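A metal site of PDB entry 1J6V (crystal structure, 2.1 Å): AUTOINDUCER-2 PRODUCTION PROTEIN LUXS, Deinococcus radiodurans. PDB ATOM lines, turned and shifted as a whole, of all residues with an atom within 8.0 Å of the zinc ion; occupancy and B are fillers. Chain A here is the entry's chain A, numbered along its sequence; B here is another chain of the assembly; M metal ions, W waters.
O of Pro 118 lies within hydrogen-bond range of ND1 of His 61 (2.6 Å).
A ring nitrogen (ND1) of His 57 is in hydrogen-bond range of the backbone carbonyl oxygen (O) of Asp 130, 2.8 Å away.
The side-chain sulfur (SG) of Cys 125 sits close to a ring nitrogen (NE2) of His 131 (3.6 Å).
The side-chain sulfur (SG) of Cys 125 lies close to the backbone NH (N) of Asn 127, 3.5 Å away.
The side-chain sulfur (SG) of Cys 125 sits close to the backbone NH (N) of Tyr 128 (3.5 Å).
The backbone carbonyl oxygen (O) of Cys 125 sits at hydrogen-bond distance from the side-chain amide nitrogen (ND2) of Asn 47 of chain B, at 2.8 Å.
Three residues have an atom within 4 Å of the zinc ion: His 57, His 61 and Cys 125.
The nearest printed residue that does not touch the zinc ion is His 131 (4.02 Å).
The zinc ion is bound by NE2 of His 61 (2.2 Å), NE2 of His 57 (2.2 Å), SG of Cys 125 (2.3 Å) and water W1 (2.4 Å).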
ATOM      1  N   HIS A  57       5.313 -11.835 -19.865  1.00  0.00           N
ATOM      2  CA  HIS A  57       5.958 -12.757 -20.793  1.00  0.00           C
ATOM      3  C   HIS A  57       5.575 -12.356 -22.235  1.00  0.00           C
ATOM      4  O   HIS A  57       6.419 -12.296 -23.124  1.00  0.00           O
ATOM      5  CB  HIS A  57       5.480 -14.172 -20.509  1.00  0.00           C
ATOM      6  CG  HIS A  57       6.143 -15.225 -21.343  1.00  0.00           C
ATOM      7  ND1 HIS A  57       5.679 -16.519 -21.415  1.00  0.00           N
ATOM      8  CD2 HIS A  57       7.242 -15.175 -22.120  1.00  0.00           C
ATOM      9  CE1 HIS A  57       6.469 -17.227 -22.209  1.00  0.00           C
ATOM     10  NE2 HIS A  57       7.430 -16.434 -22.646  1.00  0.00           N
ATOM     11  N   THR A  58       4.281 -12.097 -22.465  1.00  0.00           N
ATOM     12  CA  THR A  58       3.788 -11.690 -23.786  1.00  0.00           C
ATOM     13  C   THR A  58       4.360 -10.321 -24.166  1.00  0.00           C
ATOM     14  O   THR A  58       4.745 -10.101 -25.309  1.00  0.00           O
ATOM     15  CB  THR A  58       2.246 -11.612 -23.795  1.00  0.00           C
ATOM     16  OG1 THR A  58       1.727 -12.925 -23.605  1.00  0.00           O
ATOM     17  CG2 THR A  58       1.711 -11.036 -25.129  1.00  0.00           C
ATOM     18  N   GLU A  60       7.096  -9.202 -23.313  1.00  0.00           N
ATOM     19  CA  GLU A  60       8.489  -9.473 -23.649  1.00  0.00           C
ATOM     20  C   GLU A  60       8.565  -9.882 -25.119  1.00  0.00           C
ATOM     21  O   GLU A  60       9.412  -9.385 -25.864  1.00  0.00           O
ATOM     22  CB  GLU A  60       9.046 -10.599 -22.780  1.00  0.00           C
ATOM     23  CG  GLU A  60      10.476 -11.042 -23.136  1.00  0.00           C
ATOM     24  CD  GLU A  60      10.876 -12.350 -22.462  1.00  0.00           C
ATOM     25  OE1 GLU A  60      10.203 -13.379 -22.696  1.00  0.00           O
ATOM     26  OE2 GLU A  60      11.869 -12.356 -21.699  1.00  0.00           O
ATOM     27  N   HIS A  61       7.678 -10.781 -25.531  1.00  0.00           N
ATOM     28  CA  HIS A  61       7.641 -11.236 -26.908  1.00  0.00           C
ATOM     29  C   HIS A  61       7.357 -10.134 -27.912  1.00  0.00           C
ATOM     30  O   HIS A  61       7.975 -10.091 -28.974  1.00  0.00           O
ATOM     31  CB  HIS A  61       6.587 -12.341 -27.109  1.00  0.00           C
ATOM     32  CG  HIS A  61       7.072 -13.718 -26.788  1.00  0.00           C
ATOM     33  ND1 HIS A  61       6.864 -14.784 -27.628  1.00  0.00           N
ATOM     34  CD2 HIS A  61       7.730 -14.200 -25.708  1.00  0.00           C
ATOM     35  CE1 HIS A  61       7.378 -15.878 -27.073  1.00  0.00           C
ATOM     36  NE2 HIS A  61       7.901 -15.547 -25.918  1.00  0.00           N
ATOM     37  N   ILE A 117       0.467 -13.992 -30.985  1.00  0.00           N
ATOM     38  CA  ILE A 117       1.664 -13.540 -30.302  1.00  0.00           C
ATOM     39  C   ILE A 117       2.825 -14.155 -31.064  1.00  0.00           C
ATOM     40  O   ILE A 117       2.823 -15.355 -31.343  1.00  0.00           O
ATOM     41  CB  ILE A 117       1.711 -14.052 -28.867  1.00  0.00           C
ATOM     42  CG1 ILE A 117       0.514 -13.487 -28.102  1.00  0.00           C
ATOM     43  CG2 ILE A 117       3.032 -13.670 -28.226  1.00  0.00           C
ATOM     44  CD1 ILE A 117       0.340 -14.098 -26.725  1.00  0.00           C
ATOM     45  N   PRO A 118       3.844 -13.354 -31.414  1.00  0.00           N
ATOM     46  CA  PRO A 118       4.961 -13.952 -32.150  1.00  0.00           C
ATOM     47  C   PRO A 118       5.807 -14.931 -31.327  1.00  0.00           C
ATOM     48  O   PRO A 118       5.975 -14.776 -30.114  1.00  0.00           O
ATOM     49  CB  PRO A 118       5.750 -12.736 -32.634  1.00  0.00           C
ATOM     50  CG  PRO A 118       5.466 -11.688 -31.597  1.00  0.00           C
ATOM     51  CD  PRO A 118       3.992 -11.885 -31.305  1.00  0.00           C
ATOM     52  N   GLY A 119       6.298 -15.974 -32.013  1.00  0.00           N
ATOM     53  CA  GLY A 119       7.159 -16.968 -31.399  1.00  0.00           C
ATOM     54  C   GLY A 119       6.587 -17.842 -30.294  1.00  0.00           C
ATOM     55  O   GLY A 119       7.325 -18.268 -29.422  1.00  0.00           O
ATOM     56  N   VAL A 120       5.282 -18.117 -30.325  1.00  0.00           N
ATOM     57  CA  VAL A 120       4.687 -18.943 -29.288  1.00  0.00           C
ATOM     58  C   VAL A 120       4.488 -20.400 -29.721  1.00  0.00           C
ATOM     59  O   VAL A 120       3.531 -20.729 -30.424  1.00  0.00           O
ATOM     60  CB  VAL A 120       3.342 -18.351 -28.828  1.00  0.00           C
ATOM     61  CG1 VAL A 120       2.725 -19.215 -27.751  1.00  0.00           C
ATOM     62  CG2 VAL A 120       3.556 -16.934 -28.293  1.00  0.00           C
ATOM     63  N   SER A 121       5.408 -21.268 -29.290  1.00  0.00           N
ATOM     64  CA  SER A 121       5.353 -22.699 -29.578  1.00  0.00           C
ATOM     65  C   SER A 121       6.429 -23.391 -28.758  1.00  0.00           C
ATOM     66  O   SER A 121       7.317 -22.731 -28.200  1.00  0.00           O
ATOM     67  CB  SER A 121       5.583 -22.972 -31.074  1.00  0.00           C
ATOM     68  OG  SER A 121       6.944 -22.810 -31.421  1.00  0.00           O
ATOM     69  N   GLU A 124      10.005 -22.472 -30.255  1.00  0.00           N
ATOM     70  CA  GLU A 124      10.542 -21.116 -30.085  1.00  0.00           C
ATOM     71  C   GLU A 124      10.387 -20.446 -28.728  1.00  0.00           C
ATOM     72  O   GLU A 124      10.937 -19.373 -28.519  1.00  0.00           O
ATOM     73  CB  GLU A 124       9.892 -20.192 -31.120  1.00  0.00           C
ATOM     74  CG  GLU A 124       9.674 -20.818 -32.480  1.00  0.00           C
ATOM     75  CD  GLU A 124       8.562 -20.118 -33.246  1.00  0.00           C
ATOM     76  OE1 GLU A 124       8.815 -19.028 -33.815  1.00  0.00           O
ATOM     77  OE2 GLU A 124       7.428 -20.650 -33.263  1.00  0.00           O
ATOM     78  N   CYS A 125       9.626 -21.044 -27.831  1.00  0.00           N
ATOM     79  CA  CYS A 125       9.380 -20.441 -26.517  1.00  0.00           C
ATOM     80  C   CYS A 125       9.561 -21.403 -25.350  1.00  0.00           C
ATOM     81  O   CYS A 125       9.112 -22.544 -25.418  1.00  0.00           O
ATOM     82  CB  CYS A 125       7.964 -19.852 -26.520  1.00  0.00           C
ATOM     83  SG  CYS A 125       7.418 -19.103 -24.967  1.00  0.00           S
ATOM     84  N   GLY A 126      10.194 -20.943 -24.263  1.00  0.00           N
ATOM     85  CA  GLY A 126      10.426 -21.781 -23.098  1.00  0.00           C
ATOM     86  C   GLY A 126       9.247 -22.071 -22.163  1.00  0.00           C
ATOM     87  O   GLY A 126       9.367 -22.885 -21.241  1.00  0.00           O
ATOM     88  N   ASN A 127       8.119 -21.397 -22.378  1.00  0.00           N
ATOM     89  CA  ASN A 127       6.921 -21.602 -21.557  1.00  0.00           C
ATOM     90  C   ASN A 127       5.741 -21.131 -22.399  1.00  0.00           C
ATOM     91  O   ASN A 127       4.986 -20.247 -21.988  1.00  0.00           O
ATOM     92  CB  ASN A 127       7.007 -20.795 -20.251  1.00  0.00           C
ATOM     93  CG  ASN A 127       5.950 -21.212 -19.231  1.00  0.00           C
ATOM     94  OD1 ASN A 127       5.162 -22.120 -19.476  1.00  0.00           O
ATOM     95  ND2 ASN A 127       5.930 -20.550 -18.085  1.00  0.00           N
ATOM     96  N   TYR A 128       5.573 -21.742 -23.568  1.00  0.00           N
ATOM     97  CA  TYR A 128       4.538 -21.362 -24.520  1.00  0.00           C
ATOM     98  C   TYR A 128       3.108 -21.321 -24.008  1.00  0.00           C
ATOM     99  O   TYR A 128       2.272 -20.620 -24.569  1.00  0.00           O
ATOM    100  CB  TYR A 128       4.638 -22.232 -25.795  1.00  0.00           C
ATOM    101  CG  TYR A 128       4.144 -23.663 -25.663  1.00  0.00           C
ATOM    102  CD1 TYR A 128       2.804 -23.981 -25.884  1.00  0.00           C
ATOM    103  CD2 TYR A 128       5.031 -24.700 -25.352  1.00  0.00           C
ATOM    104  CE1 TYR A 128       2.348 -25.287 -25.798  1.00  0.00           C
ATOM    105  CE2 TYR A 128       4.586 -26.022 -25.260  1.00  0.00           C
ATOM    106  CZ  TYR A 128       3.239 -26.308 -25.486  1.00  0.00           C
ATOM    107  OH  TYR A 128       2.786 -27.602 -25.407  1.00  0.00           O
ATOM    108  N   ARG A 129       2.832 -22.033 -22.924  1.00  0.00           N
ATOM    109  CA  ARG A 129       1.493 -22.052 -22.368  1.00  0.00           C
ATOM    110  C   ARG A 129       1.208 -20.857 -21.449  1.00  0.00           C
ATOM    111  O   ARG A 129       0.061 -20.651 -21.063  1.00  0.00           O
ATOM    112  CB  ARG A 129       1.268 -23.306 -21.537  1.00  0.00           C
ATOM    113  CG  ARG A 129       1.531 -24.618 -22.242  1.00  0.00           C
ATOM    114  CD  ARG A 129       1.311 -25.762 -21.261  1.00  0.00           C
ATOM    115  NE  ARG A 129       1.717 -27.061 -21.790  1.00  0.00           N
ATOM    116  CZ  ARG A 129       2.947 -27.558 -21.703  1.00  0.00           C
ATOM    117  NH1 ARG A 129       3.916 -26.865 -21.104  1.00  0.00           N
ATOM    118  NH2 ARG A 129       3.230 -28.756 -22.207  1.00  0.00           N
ATOM    119  N   ASP A 130       2.238 -20.074 -21.106  1.00  0.00           N
ATOM    120  CA  ASP A 130       2.042 -18.954 -20.181  1.00  0.00           C
ATOM    121  C   ASP A 130       2.059 -17.587 -20.863  1.00  0.00           C
ATOM    122  O   ASP A 130       3.027 -16.844 -20.753  1.00  0.00           O
ATOM    123  CB  ASP A 130       3.119 -18.987 -19.095  1.00  0.00           C
ATOM    124  CG  ASP A 130       2.842 -18.008 -17.949  1.00  0.00           C
ATOM    125  OD1 ASP A 130       1.704 -18.013 -17.423  1.00  0.00           O
ATOM    126  OD2 ASP A 130       3.755 -17.235 -17.580  1.00  0.00           O
ATOM    127  N   HIS A 131       0.951 -17.270 -21.534  1.00  0.00           N
ATOM    128  CA  HIS A 131       0.792 -16.022 -22.276  1.00  0.00           C
ATOM    129  C   HIS A 131      -0.560 -15.351 -22.072  1.00  0.00           C
ATOM    130  O   HIS A 131      -1.555 -16.006 -21.751  1.00  0.00           O
ATOM    131  CB  HIS A 131       1.001 -16.295 -23.766  1.00  0.00           C
ATOM    132  CG  HIS A 131       2.447 -16.385 -24.161  1.00  0.00           C
ATOM    133  ND1 HIS A 131       3.240 -15.271 -24.305  1.00  0.00           N
ATOM    134  CD2 HIS A 131       3.233 -17.451 -24.431  1.00  0.00           C
ATOM    135  CE1 HIS A 131       4.462 -15.641 -24.655  1.00  0.00           C
ATOM    136  NE2 HIS A 131       4.478 -16.961 -24.741  1.00  0.00           N
ATOM    137  N   HIS B  14      13.976 -25.119 -28.889  1.00  0.00           N
ATOM    138  CA  HIS B  14      13.819 -25.382 -27.466  1.00  0.00           C
ATOM    139  C   HIS B  14      13.542 -26.823 -27.047  1.00  0.00           C
ATOM    140  O   HIS B  14      13.664 -27.147 -25.869  1.00  0.00           O
ATOM    141  CB  HIS B  14      12.731 -24.470 -26.869  1.00  0.00           C
ATOM    142  CG  HIS B  14      13.135 -23.026 -26.793  1.00  0.00           C
ATOM    143  ND1 HIS B  14      13.377 -22.260 -27.910  1.00  0.00           N
ATOM    144  CD2 HIS B  14      13.305 -22.211 -25.729  1.00  0.00           C
ATOM    145  CE1 HIS B  14      13.679 -21.034 -27.541  1.00  0.00           C
ATOM    146  NE2 HIS B  14      13.650 -20.965 -26.223  1.00  0.00           N
ATOM    147  N   ARG B  42      20.080 -21.488 -18.237  1.00  0.00           N
ATOM    148  CA  ARG B  42      18.875 -22.270 -18.069  1.00  0.00           C
ATOM    149  C   ARG B  42      18.802 -23.185 -16.845  1.00  0.00           C
ATOM    150  O   ARG B  42      19.570 -24.144 -16.722  1.00  0.00           O
ATOM    151  CB  ARG B  42      18.657 -23.089 -19.331  1.00  0.00           C
ATOM    152  CG  ARG B  42      17.311 -23.727 -19.441  1.00  0.00           C
ATOM    153  CD  ARG B  42      16.249 -22.722 -19.850  1.00  0.00           C
ATOM    154  NE  ARG B  42      16.620 -22.005 -21.070  1.00  0.00           N
ATOM    155  CZ  ARG B  42      15.772 -21.358 -21.858  1.00  0.00           C
ATOM    156  NH1 ARG B  42      14.466 -21.327 -21.577  1.00  0.00           N
ATOM    157  NH2 ARG B  42      16.230 -20.689 -22.922  1.00  0.00           N
ATOM    158  N   ASN B  47       9.528 -25.604 -21.075  1.00  0.00           N
ATOM    159  CA  ASN B  47       8.173 -26.161 -21.086  1.00  0.00           C
ATOM    160  C   ASN B  47       7.862 -27.351 -20.195  1.00  0.00           C
ATOM    161  O   ASN B  47       6.874 -28.063 -20.424  1.00  0.00           O
ATOM    162  CB  ASN B  47       7.770 -26.466 -22.538  1.00  0.00           C
ATOM    163  CG  ASN B  47       7.763 -25.215 -23.386  1.00  0.00           C
ATOM    164  OD1 ASN B  47       6.971 -24.307 -23.154  1.00  0.00           O
ATOM    165  ND2 ASN B  47       8.678 -25.133 -24.353  1.00  0.00           N
ATOM    166  N   MET B  80      14.196 -14.505 -17.334  1.00  0.00           N
ATOM    167  CA  MET B  80      13.578 -14.581 -18.655  1.00  0.00           C
ATOM    168  C   MET B  80      12.073 -14.554 -18.421  1.00  0.00           C
ATOM    169  O   MET B  80      11.601 -14.983 -17.371  1.00  0.00           O
ATOM    170  CB  MET B  80      13.940 -15.885 -19.357  1.00  0.00           C
ATOM    171  CG  MET B  80      15.407 -16.254 -19.268  1.00  0.00           C
ATOM    172  SD  MET B  80      15.790 -17.713 -20.468  1.00  0.00           S
ATOM    173  CE  MET B  80      15.249 -19.201 -19.427  1.00  0.00           C
ATOM    174  N   GLY B  81      11.320 -14.062 -19.397  1.00  0.00           N
ATOM    175  CA  GLY B  81       9.885 -14.008 -19.258  1.00  0.00           C
ATOM    176  C   GLY B  81       9.311 -15.409 -19.132  1.00  0.00           C
ATOM    177  O   GLY B  81       8.274 -15.595 -18.496  1.00  0.00           O
ATOM    178  N   CYS B  82       9.994 -16.394 -19.715  1.00  0.00           N
ATOM    179  CA  CYS B  82       9.500 -17.772 -19.648  1.00  0.00           C
ATOM    180  C   CYS B  82       9.752 -18.418 -18.278  1.00  0.00           C
ATOM    181  O   CYS B  82       9.242 -19.504 -18.005  1.00  0.00           O
ATOM    182  CB  CYS B  82      10.123 -18.614 -20.768  1.00  0.00           C
ATOM    183  SG  CYS B  82      11.950 -18.706 -20.819  1.00  0.00           S
ATOM    184  N   ARG B  83      10.535 -17.752 -17.433  1.00  0.00           N
ATOM    185  CA  ARG B  83      10.840 -18.231 -16.089  1.00  0.00           C
ATOM    186  C   ARG B  83      11.497 -19.612 -15.932  1.00  0.00           C
ATOM    187  O   ARG B  83      11.307 -20.279 -14.922  1.00  0.00           O
ATOM    188  CB  ARG B  83       9.569 -18.147 -15.209  1.00  0.00           C
ATOM    189  CG  ARG B  83       9.120 -16.688 -14.995  1.00  0.00           C
ATOM    190  CD  ARG B  83       7.880 -16.539 -14.137  1.00  0.00           C
ATOM    191  NE  ARG B  83       6.673 -17.038 -14.791  1.00  0.00           N
ATOM    192  CZ  ARG B  83       5.904 -18.006 -14.298  1.00  0.00           C
ATOM    193  NH1 ARG B  83       6.220 -18.573 -13.145  1.00  0.00           N
ATOM    194  NH2 ARG B  83       4.816 -18.395 -14.953  1.00  0.00           N
HETATM  195 ZN    ZN M   1       8.492 -17.069 -24.492  1.00  0.00          ZN
HETATM  196  O   HOH W   1      10.875 -17.451 -24.276  1.00  0.00           O
